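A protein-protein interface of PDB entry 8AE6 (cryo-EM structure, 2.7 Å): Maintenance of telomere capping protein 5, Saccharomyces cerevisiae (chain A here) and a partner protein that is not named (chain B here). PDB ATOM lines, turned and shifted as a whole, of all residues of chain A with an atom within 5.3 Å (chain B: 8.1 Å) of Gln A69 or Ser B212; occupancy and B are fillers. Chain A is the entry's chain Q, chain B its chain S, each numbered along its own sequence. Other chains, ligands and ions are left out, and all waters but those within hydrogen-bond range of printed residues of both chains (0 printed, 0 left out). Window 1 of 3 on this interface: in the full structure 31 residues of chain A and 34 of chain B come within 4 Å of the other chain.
The side-chain amide oxygen (OD1) of Asn B210 sits at hydrogen-bond distance from the side-chain amide nitrogen (ND2) of Asn A28 (3.3 Å).
NH1 of Arg A44 sits at hydrogen-bond distance from O of Phe B8 (2.8 Å).
The backbone NH of Gly B7 sits close to the guanidinium group of Arg A44, 3.4 Å away.
The indole nitrogen of Trp A68 lies within hydrogen-bond range of the backbone carbonyl oxygen of Ile B228, 2.6 Å away.
The backbone carbonyl oxygen of Asn B210 lies close to the backbone carbonyl oxygen of Val A70, at 3.4 Å.
Of the printed residues of chain B, Gln A69 touches Asn B209 (3.9 Å), Asn B210 (3.6 Å) and Ser B212 (3.6 Å).
Ser B212 touches two residues of chain A.
Printed residues of chain A within 4 Å of Ile B228: Trp A68.
Of the printed residues of chain B, Arg A44 touches Gly B7 (3.4 Å) and Phe B8 (2.8 Å).
Of the printed residues of chain A, Gly B7 touches Arg A44 (3.4 Å).
Of the printed residues of chain A, Phe B229 touches Trp A68.
The nearest residue of chain A that does not touch Ser B212 is Pro A67 (4.7 Å).
Printed residues of chain B that touch a printed residue of chain A: Gly B7, Phe B8, Asn B209, Asn B210, Tyr B211, Ser B212, Lys B227, Ile B228 and Phe B229.
Hydrophobic or aromatic side chains of chain B that line the printed part of chain A: Phe B8, Tyr B211 and Phe B229.
Along chain B the printed residues that touch a printed residue of chain A span positions 7 to 229.
Of the 9 printed residues of chain A, 7 touch a printed residue of chain B.
Among the printed residues, 14 pairs touch across the chains.
Among the printed residues, no Asp or Glu carboxylate lies within 4 Å of a Lys or Arg side-chain nitrogen of the other chain.
The backbone carbonyl oxygen of Phe B205 lies close to the side-chain amide oxygen of Asn B209 (3.1 Å).
N of Ile B228 is in hydrogen-bond range of O of Ser B212, 3.2 Å away.
O of Asp B207 sits at hydrogen-bond distance from N of Ser B212, 3.3 Å away.
The backbone carbonyl oxygen (O) of Gln B206 sits close to the side-chain amide nitrogen (ND2) of Asn B210 (3.1 Å).
NZ of Lys B227 lies within salt-bridge range of OE2 of Glu B213 (3.0 Å).
The side-chain amide nitrogen of Asn A28 sits at hydrogen-bond distance from the backbone carbonyl oxygen of Val A70 (2.9 Å).
Pro A67 touches Phe B8.
Trp A68 touches Phe B8 (CD1 to CE2, 3.8 Å).
Trp A68 touches Ser B212 (CD1 to CB, 3.6 Å).
Trp A68 touches Lys B227 (NE1 to CE, 3.6 Å).
Trp A68 touches Phe B229 (CZ2 to CE1, 3.96 Å).
Gln A69 touches Asn B209.
Gln A69 touches Asn B210.
OG of Ser B212 touches N of Gln A69, 3.6 Å away.
Ala A71 touches Tyr B211.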
ATOM      1  N   GLY A  26     -34.856   4.886  33.542  1.00  0.00           N
ATOM      2  CA  GLY A  26     -33.939   5.988  33.337  1.00  0.00           C
ATOM      3  C   GLY A  26     -34.628   7.332  33.297  1.00  0.00           C
ATOM      4  O   GLY A  26     -34.632   8.005  32.264  1.00  0.00           O
ATOM      5  N   ASN A  28     -34.973  11.223  34.309  1.00  0.00           N
ATOM      6  CA  ASN A  28     -34.021  12.289  34.585  1.00  0.00           C
ATOM      7  C   ASN A  28     -34.623  13.473  35.330  1.00  0.00           C
ATOM      8  O   ASN A  28     -33.869  14.263  35.907  1.00  0.00           O
ATOM      9  CB  ASN A  28     -33.399  12.784  33.274  1.00  0.00           C
ATOM     10  CG  ASN A  28     -32.047  13.428  33.477  1.00  0.00           C
ATOM     11  OD1 ASN A  28     -31.201  12.907  34.203  1.00  0.00           O
ATOM     12  ND2 ASN A  28     -31.831  14.567  32.831  1.00  0.00           N
ATOM     13  N   SER A  43     -39.051  10.790  31.354  1.00  0.00           N
ATOM     14  CA  SER A  43     -37.974  10.100  30.656  1.00  0.00           C
ATOM     15  C   SER A  43     -38.082  10.328  29.159  1.00  0.00           C
ATOM     16  O   SER A  43     -38.924  11.108  28.698  1.00  0.00           O
ATOM     17  CB  SER A  43     -37.995   8.601  30.947  1.00  0.00           C
ATOM     18  OG  SER A  43     -39.234   8.027  30.570  1.00  0.00           O
ATOM     19  N   ARG A  44     -37.233   9.648  28.390  1.00  0.00           N
ATOM     20  CA  ARG A  44     -37.300   9.731  26.940  1.00  0.00           C
ATOM     21  C   ARG A  44     -38.535   9.038  26.381  1.00  0.00           C
ATOM     22  O   ARG A  44     -38.947   9.344  25.258  1.00  0.00           O
ATOM     23  CB  ARG A  44     -36.040   9.123  26.328  1.00  0.00           C
ATOM     24  CG  ARG A  44     -34.784   9.926  26.598  1.00  0.00           C
ATOM     25  CD  ARG A  44     -33.546   9.168  26.160  1.00  0.00           C
ATOM     26  NE  ARG A  44     -33.002   8.351  27.237  1.00  0.00           N
ATOM     27  CZ  ARG A  44     -31.711   8.274  27.537  1.00  0.00           C
ATOM     28  NH1 ARG A  44     -30.802   8.955  26.860  1.00  0.00           N
ATOM     29  NH2 ARG A  44     -31.326   7.494  28.543  1.00  0.00           N
ATOM     30  N   PRO A  67     -35.593  10.851  21.267  1.00  0.00           N
ATOM     31  CA  PRO A  67     -34.242  10.302  21.448  1.00  0.00           C
ATOM     32  C   PRO A  67     -33.379  11.098  22.408  1.00  0.00           C
ATOM     33  O   PRO A  67     -32.452  10.524  22.996  1.00  0.00           O
ATOM     34  CB  PRO A  67     -33.657  10.329  20.031  1.00  0.00           C
ATOM     35  CG  PRO A  67     -34.409  11.390  19.333  1.00  0.00           C
ATOM     36  CD  PRO A  67     -35.785  11.410  19.919  1.00  0.00           C
ATOM     37  N   TRP A  68     -33.650  12.386  22.591  1.00  0.00           N
ATOM     38  CA  TRP A  68     -32.849  13.228  23.463  1.00  0.00           C
ATOM     39  C   TRP A  68     -33.339  13.137  24.901  1.00  0.00           C
ATOM     40  O   TRP A  68     -34.523  12.904  25.160  1.00  0.00           O
ATOM     41  CB  TRP A  68     -32.884  14.678  22.987  1.00  0.00           C
ATOM     42  CG  TRP A  68     -32.358  14.854  21.603  1.00  0.00           C
ATOM     43  CD1 TRP A  68     -31.054  14.960  21.233  1.00  0.00           C
ATOM     44  CD2 TRP A  68     -33.126  14.948  20.399  1.00  0.00           C
ATOM     45  NE1 TRP A  68     -30.958  15.115  19.872  1.00  0.00           N
ATOM     46  CE2 TRP A  68     -32.217  15.112  19.337  1.00  0.00           C
ATOM     47  CE3 TRP A  68     -34.495  14.913  20.116  1.00  0.00           C
ATOM     48  CZ2 TRP A  68     -32.631  15.236  18.015  1.00  0.00           C
ATOM     49  CZ3 TRP A  68     -34.902  15.036  18.803  1.00  0.00           C
ATOM     50  CH2 TRP A  68     -33.974  15.197  17.770  1.00  0.00           C
ATOM     51  N   GLN A  69     -32.413  13.320  25.836  1.00  0.00           N
ATOM     52  CA  GLN A  69     -32.737  13.204  27.252  1.00  0.00           C
ATOM     53  C   GLN A  69     -33.562  14.400  27.708  1.00  0.00           C
ATOM     54  O   GLN A  69     -33.249  15.547  27.375  1.00  0.00           O
ATOM     55  CB  GLN A  69     -31.451  13.098  28.072  1.00  0.00           C
ATOM     56  CG  GLN A  69     -31.668  12.918  29.560  1.00  0.00           C
ATOM     57  CD  GLN A  69     -32.000  11.491  29.930  1.00  0.00           C
ATOM     58  OE1 GLN A  69     -33.169  11.118  30.023  1.00  0.00           O
ATOM     59  NE2 GLN A  69     -30.973  10.683  30.149  1.00  0.00           N
ATOM     60  N   VAL A  70     -34.624  14.129  28.470  1.00  0.00           N
ATOM     61  CA  VAL A  70     -35.447  15.203  29.006  1.00  0.00           C
ATOM     62  C   VAL A  70     -34.697  15.910  30.130  1.00  0.00           C
ATOM     63  O   VAL A  70     -33.866  15.318  30.833  1.00  0.00           O
ATOM     64  CB  VAL A  70     -36.807  14.672  29.493  1.00  0.00           C
ATOM     65  CG1 VAL A  70     -37.605  14.133  28.318  1.00  0.00           C
ATOM     66  CG2 VAL A  70     -36.620  13.599  30.544  1.00  0.00           C
ATOM     67  N   ALA A  71     -34.977  17.203  30.288  1.00  0.00           N
ATOM     68  CA  ALA A  71     -34.261  18.040  31.241  1.00  0.00           C
ATOM     69  C   ALA A  71     -35.050  18.270  32.525  1.00  0.00           C
ATOM     70  O   ALA A  71     -34.576  17.943  33.617  1.00  0.00           O
ATOM     71  CB  ALA A  71     -33.917  19.380  30.589  1.00  0.00           C
ATOM     72  N   GLY B   7     -32.481   5.989  24.886  1.00  0.00           N
ATOM     73  CA  GLY B   7     -32.101   6.434  23.558  1.00  0.00           C
ATOM     74  C   GLY B   7     -30.603   6.552  23.374  1.00  0.00           C
ATOM     75  O   GLY B   7     -30.003   5.799  22.606  1.00  0.00           O
ATOM     76  N   PHE B   8     -29.995   7.502  24.078  1.00  0.00           N
ATOM     77  CA  PHE B   8     -28.563   7.744  24.005  1.00  0.00           C
ATOM     78  C   PHE B   8     -27.905   7.321  25.310  1.00  0.00           C
ATOM     79  O   PHE B   8     -28.418   7.605  26.397  1.00  0.00           O
ATOM     80  CB  PHE B   8     -28.267   9.217  23.725  1.00  0.00           C
ATOM     81  CG  PHE B   8     -28.797   9.699  22.410  1.00  0.00           C
ATOM     82  CD1 PHE B   8     -28.792   8.871  21.303  1.00  0.00           C
ATOM     83  CD2 PHE B   8     -29.301  10.981  22.281  1.00  0.00           C
ATOM     84  CE1 PHE B   8     -29.281   9.310  20.092  1.00  0.00           C
ATOM     85  CE2 PHE B   8     -29.790  11.426  21.072  1.00  0.00           C
ATOM     86  CZ  PHE B   8     -29.781  10.591  19.977  1.00  0.00           C
ATOM     87  N   VAL B   9     -26.775   6.636  25.193  1.00  0.00           N
ATOM     88  CA  VAL B   9     -26.079   6.121  26.377  1.00  0.00           C
ATOM     89  C   VAL B   9     -25.410   7.274  27.118  1.00  0.00           C
ATOM     90  O   VAL B   9     -24.845   8.178  26.475  1.00  0.00           O
ATOM     91  CB  VAL B   9     -25.069   5.038  25.967  1.00  0.00           C
ATOM     92  CG1 VAL B   9     -24.097   5.541  24.897  1.00  0.00           C
ATOM     93  CG2 VAL B   9     -24.314   4.501  27.178  1.00  0.00           C
ATOM     94  N   PRO B  10     -25.517   7.344  28.442  1.00  0.00           N
ATOM     95  CA  PRO B  10     -24.757   8.353  29.183  1.00  0.00           C
ATOM     96  C   PRO B  10     -23.268   8.046  29.174  1.00  0.00           C
ATOM     97  O   PRO B  10     -22.846   6.890  29.127  1.00  0.00           O
ATOM     98  CB  PRO B  10     -25.334   8.267  30.598  1.00  0.00           C
ATOM     99  CG  PRO B  10     -25.948   6.918  30.677  1.00  0.00           C
ATOM    100  CD  PRO B  10     -26.461   6.620  29.308  1.00  0.00           C
ATOM    101  N   TYR B 104     -22.528   9.027  19.286  1.00  0.00           N
ATOM    102  CA  TYR B 104     -21.535   9.873  19.932  1.00  0.00           C
ATOM    103  C   TYR B 104     -20.251  10.014  19.132  1.00  0.00           C
ATOM    104  O   TYR B 104     -19.474  10.935  19.403  1.00  0.00           O
ATOM    105  CB  TYR B 104     -21.201   9.320  21.316  1.00  0.00           C
ATOM    106  CG  TYR B 104     -22.227   9.661  22.363  1.00  0.00           C
ATOM    107  CD1 TYR B 104     -23.332   8.850  22.561  1.00  0.00           C
ATOM    108  CD2 TYR B 104     -22.092  10.792  23.151  1.00  0.00           C
ATOM    109  CE1 TYR B 104     -24.276   9.157  23.513  1.00  0.00           C
ATOM    110  CE2 TYR B 104     -23.030  11.107  24.110  1.00  0.00           C
ATOM    111  CZ  TYR B 104     -24.119  10.284  24.287  1.00  0.00           C
ATOM    112  OH  TYR B 104     -25.060  10.595  25.242  1.00  0.00           O
ATOM    113  N   ILE B 204     -19.223  19.400  29.607  1.00  0.00           N
ATOM    114  CA  ILE B 204     -19.497  18.454  28.523  1.00  0.00           C
ATOM    115  C   ILE B 204     -20.194  17.215  29.066  1.00  0.00           C
ATOM    116  O   ILE B 204     -21.220  16.775  28.530  1.00  0.00           O
ATOM    117  CB  ILE B 204     -18.194  18.080  27.787  1.00  0.00           C
ATOM    118  CG1 ILE B 204     -17.730  19.207  26.872  1.00  0.00           C
ATOM    119  CG2 ILE B 204     -18.389  16.829  26.950  1.00  0.00           C
ATOM    120  CD1 ILE B 204     -16.444  18.908  26.148  1.00  0.00           C
ATOM    121  N   PHE B 205     -19.676  16.677  30.178  1.00  0.00           N
ATOM    122  CA  PHE B 205     -20.228  15.474  30.790  1.00  0.00           C
ATOM    123  C   PHE B 205     -21.682  15.670  31.197  1.00  0.00           C
ATOM    124  O   PHE B 205     -22.563  14.913  30.774  1.00  0.00           O
ATOM    125  CB  PHE B 205     -19.379  15.093  32.002  1.00  0.00           C
ATOM    126  CG  PHE B 205     -19.735  13.774  32.616  1.00  0.00           C
ATOM    127  CD1 PHE B 205     -19.199  12.604  32.122  1.00  0.00           C
ATOM    128  CD2 PHE B 205     -20.583  13.709  33.708  1.00  0.00           C
ATOM    129  CE1 PHE B 205     -19.514  11.392  32.689  1.00  0.00           C
ATOM    130  CE2 PHE B 205     -20.906  12.498  34.278  1.00  0.00           C
ATOM    131  CZ  PHE B 205     -20.372  11.339  33.768  1.00  0.00           C
ATOM    132  N   GLN B 206     -21.963  16.719  31.969  1.00  0.00           N
ATOM    133  CA  GLN B 206     -23.319  16.869  32.488  1.00  0.00           C
ATOM    134  C   GLN B 206     -24.292  17.388  31.438  1.00  0.00           C
ATOM    135  O   GLN B 206     -25.477  17.040  31.484  1.00  0.00           O
ATOM    136  CB  GLN B 206     -23.312  17.760  33.720  1.00  0.00           C
ATOM    137  CG  GLN B 206     -22.729  17.045  34.909  1.00  0.00           C
ATOM    138  CD  GLN B 206     -23.623  15.927  35.407  1.00  0.00           C
ATOM    139  OE1 GLN B 206     -23.293  14.748  35.280  1.00  0.00           O
ATOM    140  NE2 GLN B 206     -24.762  16.291  35.979  1.00  0.00           N
ATOM    141  N   ASP B 207     -23.829  18.186  30.477  1.00  0.00           N
ATOM    142  CA  ASP B 207     -24.729  18.658  29.437  1.00  0.00           C
ATOM    143  C   ASP B 207     -25.078  17.546  28.457  1.00  0.00           C
ATOM    144  O   ASP B 207     -26.218  17.471  27.984  1.00  0.00           O
ATOM    145  CB  ASP B 207     -24.108  19.852  28.719  1.00  0.00           C
ATOM    146  CG  ASP B 207     -24.128  21.111  29.560  1.00  0.00           C
ATOM    147  OD1 ASP B 207     -24.737  21.092  30.649  1.00  0.00           O
ATOM    148  OD2 ASP B 207     -23.531  22.122  29.133  1.00  0.00           O
ATOM    149  N   LEU B 208     -24.126  16.666  28.141  1.00  0.00           N
ATOM    150  CA  LEU B 208     -24.442  15.544  27.270  1.00  0.00           C
ATOM    151  C   LEU B 208     -25.158  14.419  28.003  1.00  0.00           C
ATOM    152  O   LEU B 208     -25.835  13.613  27.355  1.00  0.00           O
ATOM    153  CB  LEU B 208     -23.168  15.011  26.612  1.00  0.00           C
ATOM    154  CG  LEU B 208     -22.539  15.914  25.547  1.00  0.00           C
ATOM    155  CD1 LEU B 208     -21.378  15.219  24.865  1.00  0.00           C
ATOM    156  CD2 LEU B 208     -23.575  16.350  24.531  1.00  0.00           C
ATOM    157  N   ASN B 209     -25.034  14.342  29.326  1.00  0.00           N
ATOM    158  CA  ASN B 209     -25.762  13.346  30.095  1.00  0.00           C
ATOM    159  C   ASN B 209     -27.132  13.826  30.549  1.00  0.00           C
ATOM    160  O   ASN B 209     -27.944  13.003  30.986  1.00  0.00           O
ATOM    161  CB  ASN B 209     -24.947  12.925  31.319  1.00  0.00           C
ATOM    162  CG  ASN B 209     -23.780  12.041  30.960  1.00  0.00           C
ATOM    163  OD1 ASN B 209     -23.333  12.023  29.815  1.00  0.00           O
ATOM    164  ND2 ASN B 209     -23.273  11.300  31.937  1.00  0.00           N
ATOM    165  N   ASN B 210     -27.412  15.125  30.464  1.00  0.00           N
ATOM    166  CA  ASN B 210     -28.678  15.672  30.932  1.00  0.00           C
ATOM    167  C   ASN B 210     -29.535  16.274  29.832  1.00  0.00           C
ATOM    168  O   ASN B 210     -30.754  16.342  29.992  1.00  0.00           O
ATOM    169  CB  ASN B 210     -28.428  16.745  32.000  1.00  0.00           C
ATOM    170  CG  ASN B 210     -28.138  16.151  33.357  1.00  0.00           C
ATOM    171  OD1 ASN B 210     -28.740  15.156  33.755  1.00  0.00           O
ATOM    172  ND2 ASN B 210     -27.204  16.758  34.075  1.00  0.00           N
ATOM    173  N   TYR B 211     -28.937  16.714  28.727  1.00  0.00           N
ATOM    174  CA  TYR B 211     -29.681  17.402  27.690  1.00  0.00           C
ATOM    175  C   TYR B 211     -29.457  16.830  26.300  1.00  0.00           C
ATOM    176  O   TYR B 211     -30.192  17.203  25.379  1.00  0.00           O
ATOM    177  CB  TYR B 211     -29.307  18.892  27.667  1.00  0.00           C
ATOM    178  CG  TYR B 211     -29.315  19.531  29.031  1.00  0.00           C
ATOM    179  CD1 TYR B 211     -30.502  19.870  29.651  1.00  0.00           C
ATOM    180  CD2 TYR B 211     -28.129  19.812  29.689  1.00  0.00           C
ATOM    181  CE1 TYR B 211     -30.510  20.444  30.903  1.00  0.00           C
ATOM    182  CE2 TYR B 211     -28.124  20.395  30.937  1.00  0.00           C
ATOM    183  CZ  TYR B 211     -29.318  20.711  31.539  1.00  0.00           C
ATOM    184  OH  TYR B 211     -29.320  21.293  32.782  1.00  0.00           O
ATOM    185  N   SER B 212     -28.457  15.954  26.128  1.00  0.00           N
ATOM    186  CA  SER B 212     -27.962  15.484  24.825  1.00  0.00           C
ATOM    187  C   SER B 212     -27.545  16.643  23.922  1.00  0.00           C
ATOM    188  O   SER B 212     -27.578  16.531  22.698  1.00  0.00           O
ATOM    189  CB  SER B 212     -28.977  14.582  24.118  1.00  0.00           C
ATOM    190  OG  SER B 212     -28.964  13.275  24.667  1.00  0.00           O
ATOM    191  N   GLU B 213     -27.122  17.746  24.536  1.00  0.00           N
ATOM    192  CA  GLU B 213     -26.759  18.976  23.854  1.00  0.00           C
ATOM    193  C   GLU B 213     -25.843  19.765  24.773  1.00  0.00           C
ATOM    194  O   GLU B 213     -25.868  19.590  25.991  1.00  0.00           O
ATOM    195  CB  GLU B 213     -27.987  19.818  23.499  1.00  0.00           C
ATOM    196  CG  GLU B 213     -28.608  19.544  22.149  1.00  0.00           C
ATOM    197  CD  GLU B 213     -29.737  20.498  21.858  1.00  0.00           C
ATOM    198  OE1 GLU B 213     -29.780  21.556  22.514  1.00  0.00           O
ATOM    199  OE2 GLU B 213     -30.582  20.194  20.993  1.00  0.00           O
ATOM    200  N   CYS B 214     -25.047  20.651  24.178  1.00  0.00           N
ATOM    201  CA  CYS B 214     -24.185  21.514  24.971  1.00  0.00           C
ATOM    202  C   CYS B 214     -23.840  22.764  24.177  1.00  0.00           C
ATOM    203  O   CYS B 214     -23.779  22.738  22.946  1.00  0.00           O
ATOM    204  CB  CYS B 214     -22.907  20.787  25.410  1.00  0.00           C
ATOM    205  SG  CYS B 214     -21.592  20.689  24.190  1.00  0.00           S
ATOM    206  N   ILE B 226     -22.269  20.793  20.714  1.00  0.00           N
ATOM    207  CA  ILE B 226     -22.446  19.384  20.385  1.00  0.00           C
ATOM    208  C   ILE B 226     -23.917  19.042  20.548  1.00  0.00           C
ATOM    209  O   ILE B 226     -24.510  19.333  21.588  1.00  0.00           O
ATOM    210  CB  ILE B 226     -21.573  18.483  21.281  1.00  0.00           C
ATOM    211  CG1 ILE B 226     -20.097  18.617  20.907  1.00  0.00           C
ATOM    212  CG2 ILE B 226     -22.018  17.038  21.202  1.00  0.00           C
ATOM    213  CD1 ILE B 226     -19.171  17.849  21.817  1.00  0.00           C
ATOM    214  N   LYS B 227     -24.506  18.442  19.517  1.00  0.00           N
ATOM    215  CA  LYS B 227     -25.848  17.883  19.601  1.00  0.00           C
ATOM    216  C   LYS B 227     -25.800  16.442  19.127  1.00  0.00           C
ATOM    217  O   LYS B 227     -25.304  16.163  18.032  1.00  0.00           O
ATOM    218  CB  LYS B 227     -26.842  18.685  18.765  1.00  0.00           C
ATOM    219  CG  LYS B 227     -28.163  17.992  18.520  1.00  0.00           C
ATOM    220  CD  LYS B 227     -29.254  18.995  18.216  1.00  0.00           C
ATOM    221  CE  LYS B 227     -30.624  18.348  18.261  1.00  0.00           C
ATOM    222  NZ  LYS B 227     -31.707  19.366  18.323  1.00  0.00           N
ATOM    223  N   ILE B 228     -26.317  15.535  19.946  1.00  0.00           N
ATOM    224  CA  ILE B 228     -26.287  14.110  19.645  1.00  0.00           C
ATOM    225  C   ILE B 228     -27.548  13.759  18.867  1.00  0.00           C
ATOM    226  O   ILE B 228     -28.664  13.927  19.370  1.00  0.00           O
ATOM    227  CB  ILE B 228     -26.177  13.275  20.927  1.00  0.00           C
ATOM    228  CG1 ILE B 228     -24.940  13.684  21.724  1.00  0.00           C
ATOM    229  CG2 ILE B 228     -26.127  11.802  20.593  1.00  0.00           C
ATOM    230  CD1 ILE B 228     -23.644  13.455  20.995  1.00  0.00           C
ATOM    231  N   PHE B 229     -27.370  13.275  17.645  1.00  0.00           N
ATOM    232  CA  PHE B 229     -28.459  12.890  16.768  1.00  0.00           C
ATOM    233  C   PHE B 229     -28.578  11.375  16.685  1.00  0.00           C
ATOM    234  O   PHE B 229     -27.568  10.664  16.728  1.00  0.00           O
ATOM    235  CB  PHE B 229     -28.240  13.447  15.360  1.00  0.00           C
ATOM    236  CG  PHE B 229     -28.806  14.812  15.157  1.00  0.00           C
ATOM    237  CD1 PHE B 229     -30.153  14.984  14.916  1.00  0.00           C
ATOM    238  CD2 PHE B 229     -27.991  15.924  15.202  1.00  0.00           C
ATOM    239  CE1 PHE B 229     -30.677  16.243  14.726  1.00  0.00           C
ATOM    240  CE2 PHE B 229     -28.506  17.181  15.012  1.00  0.00           C
ATOM    241  CZ  PHE B 229     -29.849  17.342  14.776  1.00  0.00           C
